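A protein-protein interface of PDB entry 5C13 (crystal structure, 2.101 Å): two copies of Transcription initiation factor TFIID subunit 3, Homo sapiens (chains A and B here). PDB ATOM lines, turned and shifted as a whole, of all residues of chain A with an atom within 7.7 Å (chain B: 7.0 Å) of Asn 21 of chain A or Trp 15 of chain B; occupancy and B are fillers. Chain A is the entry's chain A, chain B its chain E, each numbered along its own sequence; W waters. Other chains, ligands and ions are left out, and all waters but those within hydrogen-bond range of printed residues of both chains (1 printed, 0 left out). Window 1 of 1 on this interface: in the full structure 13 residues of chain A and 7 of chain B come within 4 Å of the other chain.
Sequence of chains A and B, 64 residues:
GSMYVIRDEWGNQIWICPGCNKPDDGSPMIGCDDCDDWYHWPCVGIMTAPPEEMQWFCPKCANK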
ATOM      1  N   MET A   3      -1.133  16.337  -2.720  1.00  0.00           N
ATOM      2  CA  MET A   3       0.220  16.250  -3.294  1.00  0.00           C
ATOM      3  C   MET A   3       0.822  14.824  -3.544  1.00  0.00           C
ATOM      4  O   MET A   3       0.912  13.970  -2.652  1.00  0.00           O
ATOM      5  CB  MET A   3       1.213  17.002  -2.405  1.00  0.00           C
ATOM      6  CG  MET A   3       1.096  18.523  -2.429  1.00  0.00           C
ATOM      7  SD  MET A   3       2.305  19.286  -1.344  1.00  0.00           S
ATOM      8  CE  MET A   3       3.536  19.761  -2.572  1.00  0.00           C
ATOM      9  N   TYR A   4       1.356  14.626  -4.735  1.00  0.00           N
ATOM     10  CA  TYR A   4       2.177  13.435  -4.970  1.00  0.00           C
ATOM     11  C   TYR A   4       3.503  13.597  -4.238  1.00  0.00           C
ATOM     12  O   TYR A   4       4.055  14.700  -4.245  1.00  0.00           O
ATOM     13  CB  TYR A   4       2.421  13.220  -6.474  1.00  0.00           C
ATOM     14  CG  TYR A   4       1.349  12.395  -7.200  1.00  0.00           C
ATOM     15  CD1 TYR A   4       1.299  11.006  -7.049  1.00  0.00           C
ATOM     16  CD2 TYR A   4       0.439  12.988  -8.068  1.00  0.00           C
ATOM     17  CE1 TYR A   4       0.351  10.238  -7.721  1.00  0.00           C
ATOM     18  CE2 TYR A   4      -0.518  12.220  -8.743  1.00  0.00           C
ATOM     19  CZ  TYR A   4      -0.546  10.846  -8.550  1.00  0.00           C
ATOM     20  OH  TYR A   4      -1.463  10.056  -9.197  1.00  0.00           O
ATOM     21  N   VAL A   5       4.007  12.509  -3.630  1.00  0.00           N
ATOM     22  CA  VAL A   5       5.368  12.454  -3.060  1.00  0.00           C
ATOM     23  C   VAL A   5       6.274  11.421  -3.748  1.00  0.00           C
ATOM     24  O   VAL A   5       5.984  10.229  -3.768  1.00  0.00           O
ATOM     25  CB  VAL A   5       5.324  12.141  -1.548  1.00  0.00           C
ATOM     26  CG1 VAL A   5       4.645  13.263  -0.832  1.00  0.00           C
ATOM     27  CG2 VAL A   5       4.538  10.873  -1.277  1.00  0.00           C
ATOM     28  N   ILE A   6       7.377  11.878  -4.320  1.00  0.00           N
ATOM     29  CA  ILE A   6       8.332  10.961  -4.912  1.00  0.00           C
ATOM     30  C   ILE A   6       9.350  10.515  -3.892  1.00  0.00           C
ATOM     31  O   ILE A   6       9.952  11.334  -3.202  1.00  0.00           O
ATOM     32  CB  ILE A   6       9.101  11.585  -6.063  1.00  0.00           C
ATOM     33  CG1 ILE A   6       8.150  11.883  -7.202  1.00  0.00           C
ATOM     34  CG2 ILE A   6      10.222  10.648  -6.484  1.00  0.00           C
ATOM     35  CD1 ILE A   6       8.808  12.403  -8.474  1.00  0.00           C
ATOM     36  N   TRP A  15       8.145  16.455  -2.565  1.00  0.00           N
ATOM     37  CA  TRP A  15       6.747  16.814  -2.696  1.00  0.00           C
ATOM     38  C   TRP A  15       6.509  17.595  -3.963  1.00  0.00           C
ATOM     39  O   TRP A  15       7.236  18.542  -4.248  1.00  0.00           O
ATOM     40  CB  TRP A  15       6.291  17.602  -1.505  1.00  0.00           C
ATOM     41  CG  TRP A  15       6.499  16.828  -0.288  1.00  0.00           C
ATOM     42  CD1 TRP A  15       7.685  16.608   0.347  1.00  0.00           C
ATOM     43  CD2 TRP A  15       5.498  16.173   0.488  1.00  0.00           C
ATOM     44  NE1 TRP A  15       7.484  15.838   1.465  1.00  0.00           N
ATOM     45  CE2 TRP A  15       6.148  15.554   1.570  1.00  0.00           C
ATOM     46  CE3 TRP A  15       4.116  16.052   0.374  1.00  0.00           C
ATOM     47  CZ2 TRP A  15       5.466  14.825   2.525  1.00  0.00           C
ATOM     48  CZ3 TRP A  15       3.441  15.313   1.314  1.00  0.00           C
ATOM     49  CH2 TRP A  15       4.112  14.709   2.375  1.00  0.00           C
ATOM     50  N   ILE A  16       5.485  17.181  -4.712  1.00  0.00           N
ATOM     51  CA  ILE A  16       5.230  17.687  -6.056  1.00  0.00           C
ATOM     52  C   ILE A  16       4.105  18.724  -6.087  1.00  0.00           C
ATOM     53  O   ILE A  16       3.007  18.470  -5.598  1.00  0.00           O
ATOM     54  CB  ILE A  16       4.845  16.522  -7.036  1.00  0.00           C
ATOM     55  CG1 ILE A  16       5.829  15.335  -6.902  1.00  0.00           C
ATOM     56  CG2 ILE A  16       4.753  17.027  -8.430  1.00  0.00           C
ATOM     57  CD1 ILE A  16       7.194  15.655  -7.325  1.00  0.00           C
ATOM     58  N   CYS A  17       4.388  19.883  -6.683  1.00  0.00           N
ATOM     59  CA  CYS A  17       3.352  20.845  -7.063  1.00  0.00           C
ATOM     60  C   CYS A  17       2.179  20.180  -7.786  1.00  0.00           C
ATOM     61  O   CYS A  17       2.382  19.562  -8.823  1.00  0.00           O
ATOM     62  CB  CYS A  17       3.972  21.919  -7.954  1.00  0.00           C
ATOM     63  SG  CYS A  17       2.882  23.061  -8.706  1.00  0.00           S
ATOM     64  N   PRO A  18       0.950  20.281  -7.237  1.00  0.00           N
ATOM     65  CA  PRO A  18      -0.181  19.693  -7.976  1.00  0.00           C
ATOM     66  C   PRO A  18      -0.556  20.478  -9.265  1.00  0.00           C
ATOM     67  O   PRO A  18      -1.330  20.018 -10.090  1.00  0.00           O
ATOM     68  CB  PRO A  18      -1.338  19.749  -6.966  1.00  0.00           C
ATOM     69  CG  PRO A  18      -0.738  20.080  -5.651  1.00  0.00           C
ATOM     70  CD  PRO A  18       0.534  20.820  -5.931  1.00  0.00           C
ATOM     71  N   GLY A  19       0.007  21.658  -9.440  1.00  0.00           N
ATOM     72  CA  GLY A  19      -0.312  22.452 -10.608  1.00  0.00           C
ATOM     73  C   GLY A  19       0.321  21.917 -11.863  1.00  0.00           C
ATOM     74  O   GLY A  19      -0.317  21.799 -12.906  1.00  0.00           O
ATOM     75  N   CYS A  20       1.589  21.594 -11.763  1.00  0.00           N
ATOM     76  CA  CYS A  20       2.301  21.085 -12.904  1.00  0.00           C
ATOM     77  C   CYS A  20       2.615  19.581 -12.761  1.00  0.00           C
ATOM     78  O   CYS A  20       2.774  18.870 -13.757  1.00  0.00           O
ATOM     79  CB  CYS A  20       3.568  21.917 -13.077  1.00  0.00           C
ATOM     80  SG  CYS A  20       4.753  21.733 -11.736  1.00  0.00           S
ATOM     81  N   ASN A  21       2.691  19.107 -11.515  1.00  0.00           N
ATOM     82  CA  ASN A  21       3.082  17.726 -11.207  1.00  0.00           C
ATOM     83  C   ASN A  21       4.418  17.389 -11.854  1.00  0.00           C
ATOM     84  O   ASN A  21       4.641  16.271 -12.304  1.00  0.00           O
ATOM     85  CB  ASN A  21       1.998  16.732 -11.627  1.00  0.00           C
ATOM     86  CG  ASN A  21       0.993  16.476 -10.529  1.00  0.00           C
ATOM     87  OD1 ASN A  21       1.364  16.088  -9.439  1.00  0.00           O
ATOM     88  ND2 ASN A  21      -0.289  16.704 -10.804  1.00  0.00           N
ATOM     89  N   LYS A  22       5.297  18.384 -11.906  1.00  0.00           N
ATOM     90  CA  LYS A  22       6.669  18.175 -12.313  1.00  0.00           C
ATOM     91  C   LYS A  22       7.531  18.288 -11.052  1.00  0.00           C
ATOM     92  O   LYS A  22       7.404  19.237 -10.263  1.00  0.00           O
ATOM     93  CB  LYS A  22       7.106  19.173 -13.390  1.00  0.00           C
ATOM     94  CG  LYS A  22       6.450  18.948 -14.763  1.00  0.00           C
ATOM     95  CD  LYS A  22       7.340  18.199 -15.755  1.00  0.00           C
ATOM     96  CE  LYS A  22       7.431  18.920 -17.099  1.00  0.00           C
ATOM     97  NZ  LYS A  22       8.210  18.097 -18.077  1.00  0.00           N
ATOM     98  N   PRO A  23       8.375  17.286 -10.818  1.00  0.00           N
ATOM     99  CA  PRO A  23       9.294  17.385  -9.687  1.00  0.00           C
ATOM    100  C   PRO A  23      10.410  18.403  -9.851  1.00  0.00           C
ATOM    101  O   PRO A  23      10.919  18.892  -8.852  1.00  0.00           O
ATOM    102  CB  PRO A  23       9.883  15.977  -9.605  1.00  0.00           C
ATOM    103  CG  PRO A  23       9.646  15.382 -10.937  1.00  0.00           C
ATOM    104  CD  PRO A  23       8.372  15.940 -11.404  1.00  0.00           C
ATOM    105  N   ASP A  24      10.813  18.717 -11.070  1.00  0.00           N
ATOM    106  CA  ASP A  24      11.994  19.553 -11.213  1.00  0.00           C
ATOM    107  C   ASP A  24      11.648  21.021 -11.100  1.00  0.00           C
ATOM    108  O   ASP A  24      11.224  21.663 -12.059  1.00  0.00           O
ATOM    109  CB  ASP A  24      12.696  19.249 -12.527  1.00  0.00           C
ATOM    110  CG  ASP A  24      13.468  17.952 -12.465  1.00  0.00           C
ATOM    111  OD1 ASP A  24      13.869  17.556 -11.348  1.00  0.00           O
ATOM    112  OD2 ASP A  24      13.665  17.323 -13.523  1.00  0.00           O
ATOM    113  N   ASP A  25      11.831  21.537  -9.891  1.00  0.00           N
ATOM    114  CA  ASP A  25      11.490  22.912  -9.585  1.00  0.00           C
ATOM    115  C   ASP A  25      12.637  23.839  -9.880  1.00  0.00           C
ATOM    116  O   ASP A  25      12.861  24.231 -11.024  1.00  0.00           O
ATOM    117  CB  ASP A  25      11.101  23.065  -8.109  1.00  0.00           C
ATOM    118  CG  ASP A  25      10.197  21.972  -7.638  1.00  0.00           C
ATOM    119  OD1 ASP A  25       9.414  21.481  -8.473  1.00  0.00           O
ATOM    120  OD2 ASP A  25      10.240  21.615  -6.441  1.00  0.00           O
ATOM    121  N   HIS A  40       4.223  25.730  -6.927  1.00  0.00           N
ATOM    122  CA  HIS A  40       5.095  26.763  -7.477  1.00  0.00           C
ATOM    123  C   HIS A  40       4.346  28.062  -7.701  1.00  0.00           C
ATOM    124  O   HIS A  40       3.212  28.047  -8.209  1.00  0.00           O
ATOM    125  CB  HIS A  40       5.684  26.353  -8.830  1.00  0.00           C
ATOM    126  CG  HIS A  40       6.361  25.026  -8.833  1.00  0.00           C
ATOM    127  ND1 HIS A  40       5.933  23.973  -9.615  1.00  0.00           N
ATOM    128  CD2 HIS A  40       7.475  24.597  -8.193  1.00  0.00           C
ATOM    129  CE1 HIS A  40       6.744  22.944  -9.432  1.00  0.00           C
ATOM    130  NE2 HIS A  40       7.682  23.298  -8.572  1.00  0.00           N
ATOM    131  N   CYS A  43       2.852  28.489 -11.077  1.00  0.00           N
ATOM    132  CA  CYS A  43       1.735  27.594 -11.314  1.00  0.00           C
ATOM    133  C   CYS A  43       0.469  28.153 -10.720  1.00  0.00           C
ATOM    134  O   CYS A  43      -0.604  27.709 -11.082  1.00  0.00           O
ATOM    135  CB  CYS A  43       2.022  26.185 -10.768  1.00  0.00           C
ATOM    136  SG  CYS A  43       3.402  25.430 -11.635  1.00  0.00           S
ATOM    137  N   LYS A  60      -8.469  25.111  -5.109  1.00  0.00           N
ATOM    138  CA  LYS A  60      -9.452  24.268  -4.435  1.00  0.00           C
ATOM    139  C   LYS A  60     -10.043  24.902  -3.162  1.00  0.00           C
ATOM    140  O   LYS A  60     -11.246  24.787  -2.951  1.00  0.00           O
ATOM    141  CB  LYS A  60      -8.835  22.894  -4.129  1.00  0.00           C
ATOM    142  CG  LYS A  60      -8.379  22.188  -5.411  1.00  0.00           C
ATOM    143  CD  LYS A  60      -7.561  20.945  -5.139  1.00  0.00           C
ATOM    144  CE  LYS A  60      -7.057  20.296  -6.432  1.00  0.00           C
ATOM    145  NZ  LYS A  60      -5.602  19.895  -6.313  1.00  0.00           N
ATOM    146  N   MET B   3       3.672   9.979 -22.384  1.00  0.00           N
ATOM    147  CA  MET B   3       2.558  10.240 -21.466  1.00  0.00           C
ATOM    148  C   MET B   3       1.565  11.340 -21.914  1.00  0.00           C
ATOM    149  O   MET B   3       1.942  12.465 -22.258  1.00  0.00           O
ATOM    150  CB  MET B   3       3.094  10.637 -20.101  1.00  0.00           C
ATOM    151  CG  MET B   3       3.654   9.497 -19.276  1.00  0.00           C
ATOM    152  SD  MET B   3       4.224  10.062 -17.670  1.00  0.00           S
ATOM    153  CE  MET B   3       2.944   9.467 -16.580  1.00  0.00           C
ATOM    154  N   TYR B   4       0.289  11.015 -21.792  1.00  0.00           N
ATOM    155  CA  TYR B   4      -0.774  11.987 -21.942  1.00  0.00           C
ATOM    156  C   TYR B   4      -0.777  12.851 -20.706  1.00  0.00           C
ATOM    157  O   TYR B   4      -0.535  12.332 -19.632  1.00  0.00           O
ATOM    158  CB  TYR B   4      -2.132  11.298 -22.105  1.00  0.00           C
ATOM    159  CG  TYR B   4      -2.578  10.985 -23.542  1.00  0.00           C
ATOM    160  CD1 TYR B   4      -3.141  11.964 -24.332  1.00  0.00           C
ATOM    161  CD2 TYR B   4      -2.459   9.696 -24.077  1.00  0.00           C
ATOM    162  CE1 TYR B   4      -3.566  11.687 -25.644  1.00  0.00           C
ATOM    163  CE2 TYR B   4      -2.872   9.404 -25.384  1.00  0.00           C
ATOM    164  CZ  TYR B   4      -3.435  10.413 -26.153  1.00  0.00           C
ATOM    165  OH  TYR B   4      -3.859  10.180 -27.436  1.00  0.00           O
ATOM    166  N   VAL B   5      -1.039  14.154 -20.868  1.00  0.00           N
ATOM    167  CA  VAL B   5      -1.267  15.065 -19.761  1.00  0.00           C
ATOM    168  C   VAL B   5      -2.676  15.651 -19.816  1.00  0.00           C
ATOM    169  O   VAL B   5      -3.055  16.226 -20.809  1.00  0.00           O
ATOM    170  CB  VAL B   5      -0.260  16.249 -19.767  1.00  0.00           C
ATOM    171  CG1 VAL B   5       1.128  15.771 -19.488  1.00  0.00           C
ATOM    172  CG2 VAL B   5      -0.280  16.981 -21.126  1.00  0.00           C
ATOM    173  N   ILE B   6      -3.445  15.490 -18.755  1.00  0.00           N
ATOM    174  CA  ILE B   6      -4.766  16.091 -18.662  1.00  0.00           C
ATOM    175  C   ILE B   6      -4.683  17.454 -17.972  1.00  0.00           C
ATOM    176  O   ILE B   6      -3.997  17.628 -16.954  1.00  0.00           O
ATOM    177  CB  ILE B   6      -5.758  15.234 -17.867  1.00  0.00           C
ATOM    178  CG1 ILE B   6      -6.132  14.004 -18.652  1.00  0.00           C
ATOM    179  CG2 ILE B   6      -7.011  16.015 -17.611  1.00  0.00           C
ATOM    180  CD1 ILE B   6      -7.100  13.083 -17.950  1.00  0.00           C
ATOM    181  N   ASN B  12      -5.028  22.510 -13.368  1.00  0.00           N
ATOM    182  CA  ASN B  12      -3.936  21.615 -13.001  1.00  0.00           C
ATOM    183  C   ASN B  12      -3.681  20.495 -14.011  1.00  0.00           C
ATOM    184  O   ASN B  12      -4.599  20.000 -14.666  1.00  0.00           O
ATOM    185  CB  ASN B  12      -4.201  20.961 -11.661  1.00  0.00           C
ATOM    186  CG  ASN B  12      -4.138  21.933 -10.525  1.00  0.00           C
ATOM    187  OD1 ASN B  12      -3.547  23.011 -10.638  1.00  0.00           O
ATOM    188  ND2 ASN B  12      -4.750  21.566  -9.413  1.00  0.00           N
ATOM    189  N   GLN B  13      -2.427  20.062 -14.067  1.00  0.00           N
ATOM    190  CA  GLN B  13      -1.982  19.051 -15.013  1.00  0.00           C
ATOM    191  C   GLN B  13      -1.823  17.693 -14.395  1.00  0.00           C
ATOM    192  O   GLN B  13      -1.062  17.525 -13.446  1.00  0.00           O
ATOM    193  CB  GLN B  13      -0.660  19.450 -15.599  1.00  0.00           C
ATOM    194  CG  GLN B  13      -0.752  20.478 -16.651  1.00  0.00           C
ATOM    195  CD  GLN B  13       0.612  20.779 -17.158  1.00  0.00           C
ATOM    196  OE1 GLN B  13       1.597  20.204 -16.680  1.00  0.00           O
ATOM    197  NE2 GLN B  13       0.701  21.674 -18.122  1.00  0.00           N
ATOM    198  N   ILE B  14      -2.507  16.720 -14.963  1.00  0.00           N
ATOM    199  CA  ILE B  14      -2.434  15.344 -14.477  1.00  0.00           C
ATOM    200  C   ILE B  14      -1.670  14.486 -15.490  1.00  0.00           C
ATOM    201  O   ILE B  14      -2.011  14.489 -16.674  1.00  0.00           O
ATOM    202  CB  ILE B  14      -3.867  14.794 -14.237  1.00  0.00           C
ATOM    203  CG1 ILE B  14      -4.596  15.697 -13.233  1.00  0.00           C
ATOM    204  CG2 ILE B  14      -3.846  13.334 -13.774  1.00  0.00           C
ATOM    205  CD1 ILE B  14      -6.123  15.461 -13.170  1.00  0.00           C
ATOM    206  N   TRP B  15      -0.624  13.779 -15.039  1.00  0.00           N
ATOM    207  CA  TRP B  15       0.151  12.929 -15.934  1.00  0.00           C
ATOM    208  C   TRP B  15      -0.370  11.538 -15.873  1.00  0.00           C
ATOM    209  O   TRP B  15      -0.408  10.933 -14.806  1.00  0.00           O
ATOM    210  CB  TRP B  15       1.634  12.934 -15.566  1.00  0.00           C
ATOM    211  CG  TRP B  15       2.207  14.286 -15.691  1.00  0.00           C
ATOM    212  CD1 TRP B  15       2.024  15.329 -14.831  1.00  0.00           C
ATOM    213  CD2 TRP B  15       3.037  14.767 -16.739  1.00  0.00           C
ATOM    214  NE1 TRP B  15       2.689  16.433 -15.285  1.00  0.00           N
ATOM    215  CE2 TRP B  15       3.315  16.117 -16.460  1.00  0.00           C
ATOM    216  CE3 TRP B  15       3.558  14.196 -17.901  1.00  0.00           C
ATOM    217  CZ2 TRP B  15       4.100  16.897 -17.292  1.00  0.00           C
ATOM    218  CZ3 TRP B  15       4.333  14.956 -18.710  1.00  0.00           C
ATOM    219  CH2 TRP B  15       4.598  16.303 -18.411  1.00  0.00           C
ATOM    220  N   ILE B  16      -0.701  10.992 -17.034  1.00  0.00           N
ATOM    221  CA  ILE B  16      -1.398   9.715 -17.092  1.00  0.00           C
ATOM    222  C   ILE B  16      -0.529   8.510 -17.412  1.00  0.00           C
ATOM    223  O   ILE B  16       0.192   8.504 -18.415  1.00  0.00           O
ATOM    224  CB  ILE B  16      -2.528   9.747 -18.177  1.00  0.00           C
ATOM    225  CG1 ILE B  16      -3.432  10.953 -17.962  1.00  0.00           C
ATOM    226  CG2 ILE B  16      -3.306   8.463 -18.164  1.00  0.00           C
ATOM    227  CD1 ILE B  16      -4.229  10.903 -16.689  1.00  0.00           C
ATOM    228  N   CYS B  17      -0.706   7.445 -16.635  1.00  0.00           N
ATOM    229  CA  CYS B  17      -0.141   6.125 -16.937  1.00  0.00           C
ATOM    230  C   CYS B  17      -0.357   5.656 -18.402  1.00  0.00           C
ATOM    231  O   CYS B  17      -1.482   5.555 -18.897  1.00  0.00           O
ATOM    232  CB  CYS B  17      -0.724   5.097 -15.956  1.00  0.00           C
ATOM    233  SG  CYS B  17      -0.268   3.357 -16.172  1.00  0.00           S
ATOM    234  N   LYS B  22      -5.681   5.887 -17.847  1.00  0.00           N
ATOM    235  CA  LYS B  22      -6.795   6.382 -17.066  1.00  0.00           C
ATOM    236  C   LYS B  22      -6.328   7.272 -15.893  1.00  0.00           C
ATOM    237  O   LYS B  22      -5.386   6.927 -15.165  1.00  0.00           O
ATOM    238  CB  LYS B  22      -7.635   5.211 -16.563  1.00  0.00           C
ATOM    239  CG  LYS B  22      -9.148   5.420 -16.727  1.00  0.00           C
ATOM    240  CD  LYS B  22      -9.560   5.890 -18.145  1.00  0.00           C
ATOM    241  CE  LYS B  22     -11.061   6.143 -18.268  1.00  0.00           C
ATOM    242  NZ  LYS B  22     -11.310   7.130 -19.393  1.00  0.00           N
ATOM    243  N   PRO B  23      -6.972   8.437 -15.726  1.00  0.00           N
ATOM    244  CA  PRO B  23      -6.598   9.400 -14.692  1.00  0.00           C
ATOM    245  C   PRO B  23      -6.986   9.021 -13.280  1.00  0.00           C
ATOM    246  O   PRO B  23      -6.311   9.447 -12.351  1.00  0.00           O
ATOM    247  CB  PRO B  23      -7.362  10.655 -15.105  1.00  0.00           C
ATOM    248  CG  PRO B  23      -8.479  10.157 -15.864  1.00  0.00           C
ATOM    249  CD  PRO B  23      -7.965   9.018 -16.638  1.00  0.00           C
ATOM    250  N   ASP B  25      -6.325   7.604 -10.720  1.00  0.00           N
ATOM    251  CA  ASP B  25      -5.223   6.809 -10.176  1.00  0.00           C
ATOM    252  C   ASP B  25      -5.337   6.577  -8.686  1.00  0.00           C
ATOM    253  O   ASP B  25      -5.889   5.567  -8.236  1.00  0.00           O
ATOM    254  CB  ASP B  25      -3.861   7.478 -10.431  1.00  0.00           C
ATOM    255  CG  ASP B  25      -3.726   8.035 -11.820  1.00  0.00           C
ATOM    256  OD1 ASP B  25      -4.484   7.599 -12.711  1.00  0.00           O
ATOM    257  OD2 ASP B  25      -2.829   8.888 -12.025  1.00  0.00           O
ATOM    258  N   MET B  29       2.813   4.964  -8.469  1.00  0.00           N
ATOM    259  CA  MET B  29       3.463   4.921  -9.768  1.00  0.00           C
ATOM    260  C   MET B  29       4.962   4.689  -9.621  1.00  0.00           C
ATOM    261  O   MET B  29       5.548   4.930  -8.548  1.00  0.00           O
ATOM    262  CB  MET B  29       3.189   6.224 -10.523  1.00  0.00           C
ATOM    263  CG  MET B  29       1.684   6.522 -10.666  1.00  0.00           C
ATOM    264  SD  MET B  29       1.294   7.976 -11.666  1.00  0.00           S
ATOM    265  CE  MET B  29       1.186   7.343 -13.325  1.00  0.00           C
ATOM    266  N   ASP B  36      11.716   8.011 -18.434  1.00  0.00           N
ATOM    267  CA  ASP B  36      10.961   8.745 -17.417  1.00  0.00           C
ATOM    268  C   ASP B  36       9.431   8.874 -17.621  1.00  0.00           C
ATOM    269  O   ASP B  36       8.794   9.745 -17.029  1.00  0.00           O
ATOM    270  CB  ASP B  36      11.531  10.145 -17.282  1.00  0.00           C
ATOM    271  CG  ASP B  36      11.369  10.699 -15.886  1.00  0.00           C
ATOM    272  OD1 ASP B  36      11.322   9.907 -14.905  1.00  0.00           O
ATOM    273  OD2 ASP B  36      11.291  11.938 -15.764  1.00  0.00           O
ATOM    274  N   TRP B  38       5.942   7.413 -16.361  1.00  0.00           N
ATOM    275  CA  TRP B  38       5.560   6.846 -15.060  1.00  0.00           C
ATOM    276  C   TRP B  38       4.362   5.964 -15.239  1.00  0.00           C
ATOM    277  O   TRP B  38       3.440   6.332 -15.977  1.00  0.00           O
ATOM    278  CB  TRP B  38       5.255   7.954 -14.033  1.00  0.00           C
ATOM    279  CG  TRP B  38       6.517   8.633 -13.551  1.00  0.00           C
ATOM    280  CD1 TRP B  38       7.312   9.430 -14.290  1.00  0.00           C
ATOM    281  CD2 TRP B  38       7.141   8.542 -12.250  1.00  0.00           C
ATOM    282  NE1 TRP B  38       8.392   9.850 -13.556  1.00  0.00           N
ATOM    283  CE2 TRP B  38       8.309   9.325 -12.296  1.00  0.00           C
ATOM    284  CE3 TRP B  38       6.824   7.889 -11.058  1.00  0.00           C
ATOM    285  CZ2 TRP B  38       9.154   9.493 -11.185  1.00  0.00           C
ATOM    286  CZ3 TRP B  38       7.669   8.065  -9.955  1.00  0.00           C
ATOM    287  CH2 TRP B  38       8.811   8.850 -10.035  1.00  0.00           C
ATOM    288  N   HIS B  40       1.434   3.114 -13.282  1.00  0.00           N
ATOM    289  CA  HIS B  40       0.970   2.490 -12.043  1.00  0.00           C
ATOM    290  C   HIS B  40       1.632   1.144 -11.858  1.00  0.00           C
ATOM    291  O   HIS B  40       1.776   0.382 -12.820  1.00  0.00           O
ATOM    292  CB  HIS B  40      -0.521   2.253 -12.012  1.00  0.00           C
ATOM    293  CG  HIS B  40      -1.331   3.444 -12.325  1.00  0.00           C
ATOM    294  ND1 HIS B  40      -2.179   3.490 -13.407  1.00  0.00           N
ATOM    295  CD2 HIS B  40      -1.442   4.632 -11.692  1.00  0.00           C
ATOM    296  CE1 HIS B  40      -2.777   4.667 -13.431  1.00  0.00           C
ATOM    297  NE2 HIS B  40      -2.342   5.373 -12.404  1.00  0.00           N
HETATM  298  O   HOH W   1      -0.104  13.593 -12.316  1.00  0.00           O
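The side-chain hydroxyl (OH) of Tyr 4 of chain A is in hydrogen-bond range of the side-chain carboxylate (OD2) of Asp 25 of chain B (3.4 Å).
The backbone carbonyl oxygen of Gly 19 of chain A is in hydrogen-bond range of the backbone NH of Gln 13 of chain B, at 3.0 Å.
OE1 of Gln 13 of chain B sits close to O of Cys 20 of chain A (3.4 Å).
NE1 of Trp 15 of chain B is in hydrogen-bond range of O of Cys 20 of chain A, at 2.9 Å.
The side-chain amide nitrogen (ND2) of Asn 21 of chain A is in hydrogen-bond range of the backbone carbonyl oxygen (O) of Gln 13 of chain B (2.9 Å).
O of Tyr 4 of chain A sits at hydrogen-bond distance from N of Ile 16 of chain A, 2.9 Å away.
SG of Cys 20 of chain A sits close to N of Lys 22 of chain A, at 3.4 Å.
N of Trp 38 of chain B sits at hydrogen-bond distance from SD of Met 3 of chain B, at 3.4 Å.
The backbone carbonyl oxygen (O) of Lys 22 of chain B sits close to the side-chain carboxylate (OD1) of Asp 25 of chain B (2.7 Å).
OD1 of Asp 25 of chain B lies close to O of Pro 23 of chain B (2.6 Å).
The side-chain carboxylate (OD1) of Asp 36 of chain B sits at hydrogen-bond distance from the indole nitrogen (NE1) of Trp 38 of chain B, at 3.2 Å.
Among the printed residues, pairs that only touch across the chains: Gly 19 of chain A with Asn 12 of chain B, Pro 18 of chain A with Asn 12 of chain B, Asn 21 of chain A with Trp 15 of chain B, Lys 60 of chain A with Asn 12 of chain B, Lys 22 of chain A with Trp 15 of chain B and Ile 6 of chain A with Trp 38 of chain B.
Asn 21 of chain A touches just these residues of chain B: Gln 13 and Trp 15.
Of chain A, only Cys 20 (2.9 Å), Asn 21 (3.5 Å) and Lys 22 (3.8 Å) come within 4 Å of Trp 15 of chain B.
Printed residues of chain A within 4 Å of Gln 13 of chain B: Gly 19, Cys 20 and Asn 21.
Of the printed residues of chain B, Pro 18 of chain A touches Asn 12 (3.4 Å).
Printed residues of chain B within 4 Å of Ile 6 of chain A: Trp 38 (3.9 Å).
Printed residues of chain A within 4 Å of Trp 38 of chain B: Ile 6.
Ile 6 of chain B touches none of the printed residues of chain A.
Val 5 of chain B touches none of the printed residues of chain A.
The nearest printed residue of chain A that does not touch Asp 25 of chain B is Asn 21 of chain A (8.3 Å).
Hydrophobic or aromatic side chains of chain B that line the printed part of chain A: Trp 15 and Trp 38.
Printed residues of chain A that touch a printed residue of chain B: Tyr 4, Ile 6, Pro 18, Gly 19, Cys 20, Asn 21, Lys 22 and Lys 60.
Tyr 4 of chain A touches Asp 25 of chain B, but with the chains exchanged Asp 25 of chain A does not touch Tyr 4 of chain B (17.5 Å).
Lys 22 of chain A touches Trp 15 of chain B, but with the chains exchanged Trp 15 of chain A does not touch Lys 22 of chain B (19.5 Å).
Positions printed for both chains: 3, 4, 5, 6, 15, 16, 17, 22, 23, 25 and 40.
Water W1 bridges the backbone NH of Trp 15 of chain B (2.8 Å) and the side-chain amide nitrogen of Asn 21 of chain A (3.5 Å).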
